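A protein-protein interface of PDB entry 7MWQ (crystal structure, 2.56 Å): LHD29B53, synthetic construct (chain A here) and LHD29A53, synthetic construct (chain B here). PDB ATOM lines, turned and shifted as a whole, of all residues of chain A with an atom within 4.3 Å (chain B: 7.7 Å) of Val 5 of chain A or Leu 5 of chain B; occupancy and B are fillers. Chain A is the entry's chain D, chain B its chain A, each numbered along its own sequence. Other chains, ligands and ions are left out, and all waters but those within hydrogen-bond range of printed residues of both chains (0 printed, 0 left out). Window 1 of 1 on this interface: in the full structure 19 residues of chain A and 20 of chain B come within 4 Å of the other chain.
Leu 53 of chain B touches Gln 3 of chain A. Ile 3 of chain B touches Trp 4 of chain A (O to CA, 3.2 Å). Val 5 of chain A touches Phe 4 of chain B (O to CA, 3.5 Å). Leu 6 of chain A touches Leu 5 of chain B. CD1 of Leu 6 of chain B touches CB of Ile 7 of chain A (3.6 Å). Ile 7 of chain A touches Ala 57 of chain B. Leu 5 of chain B touches Ile 9 of chain A (O to CD1, 3.9 Å). Ile 9 of chain A touches Ser 7 of chain B. His 42 of chain A touches Arg 54 of chain B. CB of Leu 64 of chain A touches CD1 of Phe 40 of chain B, 3.7 Å away.
Hydrophobic or aromatic side chains of chain B that line the printed part of chain A: Ile 3, Phe 4, Leu 5, Leu 6, Phe 40, Leu 53 and Leu 60. Of the 11 printed residues of chain A, 8 touch a printed residue of chain B. Printed residues of chain A that touch a printed residue of chain B: Gln 3, Trp 4, Val 5, Leu 6, Ile 7, Ile 9, His 42 and Leu 64. Hydrophobic or aromatic side chains of chain A that line the printed part of chain B: Trp 4, Val 5, Leu 6, Ile 7, Ile 9, His 42 and Leu 64. Along chain A the printed residues that touch a printed residue of chain B span positions 3 to 64. Among the printed residues, 19 pairs touch across the chains.
Of the printed residues of chain B, Gln 3 of chain A touches Ser 1, Ser 2, Ile 3, Glu 50 and Leu 53. Val 5 of chain A touches three residues of chain B. Leu 41 of chain A touches none of the printed residues of chain B. Ala 60 of chain A touches none of the printed residues of chain B. Of the printed residues of chain A, Ser 2 of chain B touches Gln 3. Leu 5 of chain B touches just these residues of chain A: Val 5 (2.7 Å), Leu 6 (3.7 Å), Ile 7 (2.9 Å) and Ile 9 (3.9 Å). Of the printed residues of chain A, Phe 40 of chain B touches Leu 64. Printed residues of chain A within 4 Å of Glu 50 of chain B: Gln 3. The nearest residue of chain B that does not touch Val 5 of chain A is Ala 57 of chain B (4.4 Å).
O of Ser 1 of chain B is in hydrogen-bond range of N of Gln 3 of chain A, 2.7 Å away. OG of Ser 2 of chain B lies within hydrogen-bond range of OE1 of Gln 3 of chain A, at 3.3 Å. N of Ile 3 of chain B sits at hydrogen-bond distance from O of Gln 3 of chain A, 2.7 Å away. O of Ile 3 of chain B sits at hydrogen-bond distance from N of Val 5 of chain A (2.8 Å). The backbone NH (N) of Leu 5 of chain B lies within hydrogen-bond range of the backbone carbonyl oxygen (O) of Val 5 of chain A, at 2.7 Å. O of Leu 5 of chain B sits at hydrogen-bond distance from N of Ile 7 of chain A (2.9 Å). The backbone NH of Ser 7 of chain B lies within hydrogen-bond range of the backbone carbonyl oxygen of Ile 7 of chain A (3.4 Å). OE1 of Glu 50 of chain B sits close to OE1 of Gln 3 of chain A (3.5 Å).
N of Phe 4 of chain B lies within hydrogen-bond range of O of Ile 43 of chain B (2.5 Å). The backbone carbonyl oxygen (O) of Leu 6 of chain B is in hydrogen-bond range of the backbone NH (N) of Leu 41 of chain B (2.6 Å). The side-chain carboxylate (OE2) of Glu 50 of chain B is in salt-bridge range of the guanidinium group (NE) of Arg 54 of chain B. The backbone carbonyl oxygen (O) of Leu 41 of chain A sits at hydrogen-bond distance from the backbone NH (N) of Leu 6 of chain A (2.8 Å).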
ATOM      1  N   GLN A   3      -2.795  -4.256 -31.489  1.00  0.00           N
ATOM      2  CA  GLN A   3      -3.329  -4.249 -30.134  1.00  0.00           C
ATOM      3  C   GLN A   3      -2.490  -3.325 -29.265  1.00  0.00           C
ATOM      4  O   GLN A   3      -1.257  -3.396 -29.290  1.00  0.00           O
ATOM      5  CB  GLN A   3      -3.353  -5.659 -29.534  1.00  0.00           C
ATOM      6  CG  GLN A   3      -3.883  -5.711 -28.109  1.00  0.00           C
ATOM      7  CD  GLN A   3      -3.904  -7.116 -27.542  1.00  0.00           C
ATOM      8  OE1 GLN A   3      -3.395  -8.053 -28.156  1.00  0.00           O
ATOM      9  NE2 GLN A   3      -4.498  -7.269 -26.364  1.00  0.00           N
ATOM     10  N   TRP A   4      -3.157  -2.463 -28.502  1.00  0.00           N
ATOM     11  CA  TRP A   4      -2.500  -1.561 -27.566  1.00  0.00           C
ATOM     12  C   TRP A   4      -2.938  -1.906 -26.150  1.00  0.00           C
ATOM     13  O   TRP A   4      -4.139  -1.989 -25.869  1.00  0.00           O
ATOM     14  CB  TRP A   4      -2.820  -0.098 -27.883  1.00  0.00           C
ATOM     15  CG  TRP A   4      -2.038   0.441 -29.039  1.00  0.00           C
ATOM     16  CD1 TRP A   4      -0.822   1.055 -28.990  1.00  0.00           C
ATOM     17  CD2 TRP A   4      -2.415   0.405 -30.420  1.00  0.00           C
ATOM     18  NE1 TRP A   4      -0.418   1.408 -30.255  1.00  0.00           N
ATOM     19  CE2 TRP A   4      -1.378   1.020 -31.151  1.00  0.00           C
ATOM     20  CE3 TRP A   4      -3.528  -0.084 -31.110  1.00  0.00           C
ATOM     21  CZ2 TRP A   4      -1.422   1.157 -32.536  1.00  0.00           C
ATOM     22  CZ3 TRP A   4      -3.570   0.052 -32.484  1.00  0.00           C
ATOM     23  CH2 TRP A   4      -2.524   0.669 -33.184  1.00  0.00           C
ATOM     24  N   VAL A   5      -1.965  -2.111 -25.269  1.00  0.00           N
ATOM     25  CA  VAL A   5      -2.212  -2.480 -23.881  1.00  0.00           C
ATOM     26  C   VAL A   5      -1.738  -1.324 -23.011  1.00  0.00           C
ATOM     27  O   VAL A   5      -0.533  -1.059 -22.913  1.00  0.00           O
ATOM     28  CB  VAL A   5      -1.509  -3.792 -23.510  1.00  0.00           C
ATOM     29  CG1 VAL A   5      -1.798  -4.164 -22.068  1.00  0.00           C
ATOM     30  CG2 VAL A   5      -1.947  -4.906 -24.449  1.00  0.00           C
ATOM     31  N   LEU A   6      -2.684  -0.632 -22.382  1.00  0.00           N
ATOM     32  CA  LEU A   6      -2.401   0.545 -21.569  1.00  0.00           C
ATOM     33  C   LEU A   6      -2.417   0.151 -20.097  1.00  0.00           C
ATOM     34  O   LEU A   6      -3.448  -0.294 -19.581  1.00  0.00           O
ATOM     35  CB  LEU A   6      -3.420   1.653 -21.839  1.00  0.00           C
ATOM     36  CG  LEU A   6      -3.214   2.558 -23.059  1.00  0.00           C
ATOM     37  CD1 LEU A   6      -3.234   1.776 -24.359  1.00  0.00           C
ATOM     38  CD2 LEU A   6      -4.274   3.640 -23.082  1.00  0.00           C
ATOM     39  N   ILE A   7      -1.279   0.322 -19.425  1.00  0.00           N
ATOM     40  CA  ILE A   7      -1.111  -0.091 -18.037  1.00  0.00           C
ATOM     41  C   ILE A   7      -0.647   1.108 -17.219  1.00  0.00           C
ATOM     42  O   ILE A   7       0.305   1.795 -17.602  1.00  0.00           O
ATOM     43  CB  ILE A   7      -0.111  -1.257 -17.908  1.00  0.00           C
ATOM     44  CG1 ILE A   7      -0.522  -2.417 -18.818  1.00  0.00           C
ATOM     45  CG2 ILE A   7      -0.019  -1.718 -16.463  1.00  0.00           C
ATOM     46  CD1 ILE A   7       0.453  -3.572 -18.819  1.00  0.00           C
ATOM     47  N   ILE A   9      -2.124   3.918 -16.796  1.00  0.00           N
ATOM     48  CA  ILE A   9      -2.398   5.145 -17.536  1.00  0.00           C
ATOM     49  C   ILE A   9      -3.530   5.883 -16.839  1.00  0.00           C
ATOM     50  O   ILE A   9      -4.519   5.269 -16.418  1.00  0.00           O
ATOM     51  CB  ILE A   9      -2.759   4.842 -19.003  1.00  0.00           C
ATOM     52  CG1 ILE A   9      -1.732   3.895 -19.625  1.00  0.00           C
ATOM     53  CG2 ILE A   9      -2.841   6.129 -19.808  1.00  0.00           C
ATOM     54  CD1 ILE A   9      -0.424   4.554 -19.983  1.00  0.00           C
ATOM     55  N   VAL A  40      -6.292  -2.579 -16.561  1.00  0.00           N
ATOM     56  CA  VAL A  40      -5.510  -2.588 -17.792  1.00  0.00           C
ATOM     57  C   VAL A  40      -6.467  -2.470 -18.969  1.00  0.00           C
ATOM     58  O   VAL A  40      -7.413  -3.259 -19.088  1.00  0.00           O
ATOM     59  CB  VAL A  40      -4.651  -3.861 -17.906  1.00  0.00           C
ATOM     60  CG1 VAL A  40      -3.957  -3.910 -19.254  1.00  0.00           C
ATOM     61  CG2 VAL A  40      -3.633  -3.919 -16.776  1.00  0.00           C
ATOM     62  N   LEU A  41      -6.220  -1.491 -19.835  1.00  0.00           N
ATOM     63  CA  LEU A  41      -7.067  -1.229 -20.991  1.00  0.00           C
ATOM     64  C   LEU A  41      -6.472  -1.906 -22.219  1.00  0.00           C
ATOM     65  O   LEU A  41      -5.341  -1.600 -22.615  1.00  0.00           O
ATOM     66  CB  LEU A  41      -7.216   0.273 -21.226  1.00  0.00           C
ATOM     67  CG  LEU A  41      -8.089   0.678 -22.416  1.00  0.00           C
ATOM     68  CD1 LEU A  41      -9.535   0.268 -22.183  1.00  0.00           C
ATOM     69  CD2 LEU A  41      -7.980   2.171 -22.670  1.00  0.00           C
ATOM     70  N   HIS A  42      -7.234  -2.816 -22.820  1.00  0.00           N
ATOM     71  CA  HIS A  42      -6.815  -3.535 -24.015  1.00  0.00           C
ATOM     72  C   HIS A  42      -7.560  -2.969 -25.218  1.00  0.00           C
ATOM     73  O   HIS A  42      -8.793  -3.028 -25.274  1.00  0.00           O
ATOM     74  CB  HIS A  42      -7.080  -5.033 -23.871  1.00  0.00           C
ATOM     75  CG  HIS A  42      -6.401  -5.657 -22.693  1.00  0.00           C
ATOM     76  ND1 HIS A  42      -5.184  -6.298 -22.787  1.00  0.00           N
ATOM     77  CD2 HIS A  42      -6.768  -5.739 -21.392  1.00  0.00           C
ATOM     78  CE1 HIS A  42      -4.831  -6.748 -21.595  1.00  0.00           C
ATOM     79  NE2 HIS A  42      -5.776  -6.421 -20.731  1.00  0.00           N
ATOM     80  N   ALA A  60      -0.678   8.822 -29.359  1.00  0.00           N
ATOM     81  CA  ALA A  60      -0.590   8.220 -28.031  1.00  0.00           C
ATOM     82  C   ALA A  60       0.666   8.676 -27.296  1.00  0.00           C
ATOM     83  O   ALA A  60       0.629   8.910 -26.083  1.00  0.00           O
ATOM     84  CB  ALA A  60      -0.625   6.697 -28.136  1.00  0.00           C
ATOM     85  N   LEU A  64       0.700  10.818 -23.706  1.00  0.00           N
ATOM     86  CA  LEU A  64       1.441  10.329 -22.549  1.00  0.00           C
ATOM     87  C   LEU A  64       2.571  11.276 -22.162  1.00  0.00           C
ATOM     88  O   LEU A  64       2.902  11.388 -20.976  1.00  0.00           O
ATOM     89  CB  LEU A  64       1.988   8.929 -22.826  1.00  0.00           C
ATOM     90  CG  LEU A  64       0.940   7.837 -23.050  1.00  0.00           C
ATOM     91  CD1 LEU A  64       1.603   6.497 -23.326  1.00  0.00           C
ATOM     92  CD2 LEU A  64      -0.005   7.738 -21.861  1.00  0.00           C
ATOM     93  N   SER B   1       2.587  -5.726 -33.723  1.00  0.00           N
ATOM     94  CA  SER B   1       1.210  -6.166 -33.540  1.00  0.00           C
ATOM     95  C   SER B   1       0.660  -5.707 -32.193  1.00  0.00           C
ATOM     96  O   SER B   1      -0.319  -4.967 -32.132  1.00  0.00           O
ATOM     97  CB  SER B   1       1.113  -7.689 -33.658  1.00  0.00           C
ATOM     98  OG  SER B   1      -0.222  -8.130 -33.477  1.00  0.00           O
ATOM     99  N   SER B   2       1.298  -6.149 -31.112  1.00  0.00           N
ATOM    100  CA  SER B   2       0.891  -5.799 -29.758  1.00  0.00           C
ATOM    101  C   SER B   2       1.863  -4.779 -29.184  1.00  0.00           C
ATOM    102  O   SER B   2       3.075  -5.013 -29.163  1.00  0.00           O
ATOM    103  CB  SER B   2       0.830  -7.039 -28.865  1.00  0.00           C
ATOM    104  OG  SER B   2      -0.259  -7.869 -29.227  1.00  0.00           O
ATOM    105  N   ILE B   3       1.330  -3.650 -28.721  1.00  0.00           N
ATOM    106  CA  ILE B   3       2.130  -2.563 -28.169  1.00  0.00           C
ATOM    107  C   ILE B   3       1.692  -2.343 -26.727  1.00  0.00           C
ATOM    108  O   ILE B   3       0.515  -2.062 -26.465  1.00  0.00           O
ATOM    109  CB  ILE B   3       1.987  -1.272 -28.990  1.00  0.00           C
ATOM    110  CG1 ILE B   3       2.345  -1.526 -30.457  1.00  0.00           C
ATOM    111  CG2 ILE B   3       2.866  -0.174 -28.413  1.00  0.00           C
ATOM    112  CD1 ILE B   3       2.312  -0.280 -31.321  1.00  0.00           C
ATOM    113  N   PHE B   4       2.634  -2.474 -25.796  1.00  0.00           N
ATOM    114  CA  PHE B   4       2.377  -2.253 -24.380  1.00  0.00           C
ATOM    115  C   PHE B   4       2.824  -0.848 -24.004  1.00  0.00           C
ATOM    116  O   PHE B   4       3.973  -0.468 -24.256  1.00  0.00           O
ATOM    117  CB  PHE B   4       3.103  -3.290 -23.521  1.00  0.00           C
ATOM    118  CG  PHE B   4       2.634  -4.701 -23.745  1.00  0.00           C
ATOM    119  CD1 PHE B   4       3.213  -5.490 -24.727  1.00  0.00           C
ATOM    120  CD2 PHE B   4       1.619  -5.239 -22.973  1.00  0.00           C
ATOM    121  CE1 PHE B   4       2.784  -6.788 -24.936  1.00  0.00           C
ATOM    122  CE2 PHE B   4       1.184  -6.536 -23.177  1.00  0.00           C
ATOM    123  CZ  PHE B   4       1.768  -7.312 -24.159  1.00  0.00           C
ATOM    124  N   LEU B   5       1.917  -0.077 -23.409  1.00  0.00           N
ATOM    125  CA  LEU B   5       2.199   1.287 -22.971  1.00  0.00           C
ATOM    126  C   LEU B   5       2.194   1.315 -21.448  1.00  0.00           C
ATOM    127  O   LEU B   5       1.147   1.127 -20.819  1.00  0.00           O
ATOM    128  CB  LEU B   5       1.184   2.270 -23.552  1.00  0.00           C
ATOM    129  CG  LEU B   5       1.288   2.486 -25.064  1.00  0.00           C
ATOM    130  CD1 LEU B   5       0.178   3.399 -25.561  1.00  0.00           C
ATOM    131  CD2 LEU B   5       2.655   3.044 -25.434  1.00  0.00           C
ATOM    132  N   LEU B   6       3.365   1.554 -20.861  1.00  0.00           N
ATOM    133  CA  LEU B   6       3.557   1.546 -19.417  1.00  0.00           C
ATOM    134  C   LEU B   6       3.982   2.940 -18.979  1.00  0.00           C
ATOM    135  O   LEU B   6       4.994   3.459 -19.461  1.00  0.00           O
ATOM    136  CB  LEU B   6       4.611   0.512 -19.020  1.00  0.00           C
ATOM    137  CG  LEU B   6       4.630   0.058 -17.561  1.00  0.00           C
ATOM    138  CD1 LEU B   6       3.433  -0.822 -17.281  1.00  0.00           C
ATOM    139  CD2 LEU B   6       5.923  -0.676 -17.245  1.00  0.00           C
ATOM    140  N   SER B   7       3.224   3.538 -18.060  1.00  0.00           N
ATOM    141  CA  SER B   7       3.462   4.911 -17.639  1.00  0.00           C
ATOM    142  C   SER B   7       3.649   4.984 -16.129  1.00  0.00           C
ATOM    143  O   SER B   7       3.141   4.145 -15.380  1.00  0.00           O
ATOM    144  CB  SER B   7       2.310   5.836 -18.056  1.00  0.00           C
ATOM    145  OG  SER B   7       2.666   7.199 -17.904  1.00  0.00           O
ATOM    146  N   GLU B  35      11.231   1.040 -26.160  1.00  0.00           N
ATOM    147  CA  GLU B  35      11.475   2.470 -26.309  1.00  0.00           C
ATOM    148  C   GLU B  35      11.258   3.148 -24.965  1.00  0.00           C
ATOM    149  O   GLU B  35      10.222   2.941 -24.324  1.00  0.00           O
ATOM    150  CB  GLU B  35      10.558   3.086 -27.373  1.00  0.00           C
ATOM    151  CG  GLU B  35      11.252   3.420 -28.690  1.00  0.00           C
ATOM    152  CD  GLU B  35      10.362   4.206 -29.639  1.00  0.00           C
ATOM    153  OE1 GLU B  35       9.145   3.928 -29.683  1.00  0.00           O
ATOM    154  OE2 GLU B  35      10.877   5.109 -30.331  1.00  0.00           O
ATOM    155  N   ASP B  37      11.301   6.613 -24.287  1.00  0.00           N
ATOM    156  CA  ASP B  37      10.284   7.620 -24.601  1.00  0.00           C
ATOM    157  C   ASP B  37      10.031   8.642 -23.489  1.00  0.00           C
ATOM    158  O   ASP B  37       8.950   9.252 -23.457  1.00  0.00           O
ATOM    159  CB  ASP B  37       8.960   6.951 -24.991  1.00  0.00           C
ATOM    160  CG  ASP B  37       9.059   6.175 -26.289  1.00  0.00           C
ATOM    161  OD1 ASP B  37       9.919   6.524 -27.128  1.00  0.00           O
ATOM    162  OD2 ASP B  37       8.274   5.218 -26.475  1.00  0.00           O
ATOM    163  N   PHE B  40       7.513   7.152 -20.094  1.00  0.00           N
ATOM    164  CA  PHE B  40       6.639   6.001 -20.277  1.00  0.00           C
ATOM    165  C   PHE B  40       7.335   4.989 -21.174  1.00  0.00           C
ATOM    166  O   PHE B  40       8.006   5.368 -22.134  1.00  0.00           O
ATOM    167  CB  PHE B  40       5.286   6.395 -20.883  1.00  0.00           C
ATOM    168  CG  PHE B  40       5.391   7.086 -22.210  1.00  0.00           C
ATOM    169  CD1 PHE B  40       5.578   8.457 -22.278  1.00  0.00           C
ATOM    170  CD2 PHE B  40       5.302   6.367 -23.390  1.00  0.00           C
ATOM    171  CE1 PHE B  40       5.674   9.096 -23.500  1.00  0.00           C
ATOM    172  CE2 PHE B  40       5.397   6.999 -24.610  1.00  0.00           C
ATOM    173  CZ  PHE B  40       5.583   8.364 -24.667  1.00  0.00           C
ATOM    174  N   LEU B  41       7.166   3.708 -20.856  1.00  0.00           N
ATOM    175  CA  LEU B  41       7.814   2.624 -21.581  1.00  0.00           C
ATOM    176  C   LEU B  41       6.892   2.085 -22.668  1.00  0.00           C
ATOM    177  O   LEU B  41       5.690   1.911 -22.447  1.00  0.00           O
ATOM    178  CB  LEU B  41       8.204   1.498 -20.621  1.00  0.00           C
ATOM    179  CG  LEU B  41       9.113   0.400 -21.172  1.00  0.00           C
ATOM    180  CD1 LEU B  41      10.415   0.987 -21.690  1.00  0.00           C
ATOM    181  CD2 LEU B  41       9.389  -0.653 -20.112  1.00  0.00           C
ATOM    182  N   THR B  42       7.464   1.827 -23.844  1.00  0.00           N
ATOM    183  CA  THR B  42       6.742   1.257 -24.975  1.00  0.00           C
ATOM    184  C   THR B  42       7.359  -0.093 -25.314  1.00  0.00           C
ATOM    185  O   THR B  42       8.570  -0.184 -25.547  1.00  0.00           O
ATOM    186  CB  THR B  42       6.783   2.191 -26.187  1.00  0.00           C
ATOM    187  OG1 THR B  42       6.049   3.388 -25.896  1.00  0.00           O
ATOM    188  CG2 THR B  42       6.177   1.514 -27.403  1.00  0.00           C
ATOM    189  N   ILE B  43       6.530  -1.133 -25.339  1.00  0.00           N
ATOM    190  CA  ILE B  43       6.973  -2.496 -25.607  1.00  0.00           C
ATOM    191  C   ILE B  43       6.141  -3.046 -26.755  1.00  0.00           C
ATOM    192  O   ILE B  43       4.913  -3.133 -26.647  1.00  0.00           O
ATOM    193  CB  ILE B  43       6.842  -3.398 -24.368  1.00  0.00           C
ATOM    194  CG1 ILE B  43       7.540  -2.764 -23.161  1.00  0.00           C
ATOM    195  CG2 ILE B  43       7.412  -4.779 -24.656  1.00  0.00           C
ATOM    196  CD1 ILE B  43       7.253  -3.463 -21.848  1.00  0.00           C
ATOM    197  N   GLU B  44       6.802  -3.423 -27.846  1.00  0.00           N
ATOM    198  CA  GLU B  44       6.135  -3.991 -29.012  1.00  0.00           C
ATOM    199  C   GLU B  44       6.537  -5.453 -29.149  1.00  0.00           C
ATOM    200  O   GLU B  44       7.728  -5.766 -29.251  1.00  0.00           O
ATOM    201  CB  GLU B  44       6.484  -3.218 -30.283  1.00  0.00           C
ATOM    202  CG  GLU B  44       5.675  -3.647 -31.499  1.00  0.00           C
ATOM    203  CD  GLU B  44       6.042  -2.875 -32.752  1.00  0.00           C
ATOM    204  OE1 GLU B  44       7.078  -2.177 -32.739  1.00  0.00           O
ATOM    205  OE2 GLU B  44       5.294  -2.965 -33.748  1.00  0.00           O
ATOM    206  N   GLU B  50      -2.289 -14.735 -27.471  1.00  0.00           N
ATOM    207  CA  GLU B  50      -3.059 -13.875 -26.578  1.00  0.00           C
ATOM    208  C   GLU B  50      -2.857 -14.258 -25.120  1.00  0.00           C
ATOM    209  O   GLU B  50      -2.891 -13.392 -24.241  1.00  0.00           O
ATOM    210  CB  GLU B  50      -4.543 -13.930 -26.947  1.00  0.00           C
ATOM    211  CG  GLU B  50      -5.405 -12.919 -26.208  1.00  0.00           C
ATOM    212  CD  GLU B  50      -5.056 -11.484 -26.560  1.00  0.00           C
ATOM    213  OE1 GLU B  50      -4.745 -11.217 -27.740  1.00  0.00           O
ATOM    214  OE2 GLU B  50      -5.088 -10.624 -25.655  1.00  0.00           O
ATOM    215  N   LEU B  53       0.468 -12.794 -24.174  1.00  0.00           N
ATOM    216  CA  LEU B  53       0.284 -11.349 -24.089  1.00  0.00           C
ATOM    217  C   LEU B  53      -0.396 -10.956 -22.784  1.00  0.00           C
ATOM    218  O   LEU B  53       0.019  -9.996 -22.124  1.00  0.00           O
ATOM    219  CB  LEU B  53      -0.527 -10.855 -25.288  1.00  0.00           C
ATOM    220  CG  LEU B  53       0.174 -10.893 -26.646  1.00  0.00           C
ATOM    221  CD1 LEU B  53      -0.819 -10.655 -27.771  1.00  0.00           C
ATOM    222  CD2 LEU B  53       1.293  -9.870 -26.689  1.00  0.00           C
ATOM    223  N   ARG B  54      -1.440 -11.690 -22.390  1.00  0.00           N
ATOM    224  CA  ARG B  54      -2.124 -11.387 -21.140  1.00  0.00           C
ATOM    225  C   ARG B  54      -1.316 -11.815 -19.922  1.00  0.00           C
ATOM    226  O   ARG B  54      -1.582 -11.330 -18.817  1.00  0.00           O
ATOM    227  CB  ARG B  54      -3.505 -12.043 -21.119  1.00  0.00           C
ATOM    228  CG  ARG B  54      -4.449 -11.511 -22.188  1.00  0.00           C
ATOM    229  CD  ARG B  54      -5.882 -11.958 -21.956  1.00  0.00           C
ATOM    230  NE  ARG B  54      -6.757 -11.556 -23.052  1.00  0.00           N
ATOM    231  CZ  ARG B  54      -7.331 -10.365 -23.156  1.00  0.00           C
ATOM    232  NH1 ARG B  54      -7.149  -9.428 -22.241  1.00  0.00           N
ATOM    233  NH2 ARG B  54      -8.105 -10.108 -24.207  1.00  0.00           N
ATOM    234  N   ILE B  56       1.985 -11.215 -19.901  1.00  0.00           N
ATOM    235  CA  ILE B  56       2.799 -10.007 -19.792  1.00  0.00           C
ATOM    236  C   ILE B  56       2.003  -8.894 -19.122  1.00  0.00           C
ATOM    237  O   ILE B  56       2.535  -8.135 -18.305  1.00  0.00           O
ATOM    238  CB  ILE B  56       3.316  -9.584 -21.180  1.00  0.00           C
ATOM    239  CG1 ILE B  56       4.300 -10.621 -21.726  1.00  0.00           C
ATOM    240  CG2 ILE B  56       3.962  -8.209 -21.121  1.00  0.00           C
ATOM    241  CD1 ILE B  56       4.851 -10.285 -23.100  1.00  0.00           C
ATOM    242  N   ALA B  57       0.710  -8.795 -19.441  1.00  0.00           N
ATOM    243  CA  ALA B  57      -0.114  -7.717 -18.904  1.00  0.00           C
ATOM    244  C   ALA B  57      -0.257  -7.824 -17.390  1.00  0.00           C
ATOM    245  O   ALA B  57      -0.049  -6.843 -16.667  1.00  0.00           O
ATOM    246  CB  ALA B  57      -1.487  -7.723 -19.579  1.00  0.00           C
ATOM    247  N   LYS B  58      -0.617  -9.010 -16.891  1.00  0.00           N
ATOM    248  CA  LYS B  58      -0.777  -9.184 -15.451  1.00  0.00           C
ATOM    249  C   LYS B  58       0.554  -9.068 -14.720  1.00  0.00           C
ATOM    250  O   LYS B  58       0.602  -8.548 -13.600  1.00  0.00           O
ATOM    251  CB  LYS B  58      -1.436 -10.531 -15.153  1.00  0.00           C
ATOM    252  CG  LYS B  58      -1.681 -10.796 -13.673  1.00  0.00           C
ATOM    253  CD  LYS B  58      -2.476  -9.669 -13.028  1.00  0.00           C
ATOM    254  CE  LYS B  58      -2.724  -9.945 -11.555  1.00  0.00           C
ATOM    255  NZ  LYS B  58      -3.397  -8.802 -10.881  1.00  0.00           N
ATOM    256  N   LEU B  60       3.174  -7.198 -15.725  1.00  0.00           N
ATOM    257  CA  LEU B  60       3.486  -5.773 -15.699  1.00  0.00           C
ATOM    258  C   LEU B  60       2.552  -5.012 -14.765  1.00  0.00           C
ATOM    259  O   LEU B  60       2.969  -4.034 -14.133  1.00  0.00           O
ATOM    260  CB  LEU B  60       3.429  -5.192 -17.113  1.00  0.00           C
ATOM    261  CG  LEU B  60       4.504  -5.671 -18.094  1.00  0.00           C
ATOM    262  CD1 LEU B  60       4.447  -4.866 -19.385  1.00  0.00           C
ATOM    263  CD2 LEU B  60       5.882  -5.592 -17.466  1.00  0.00           C
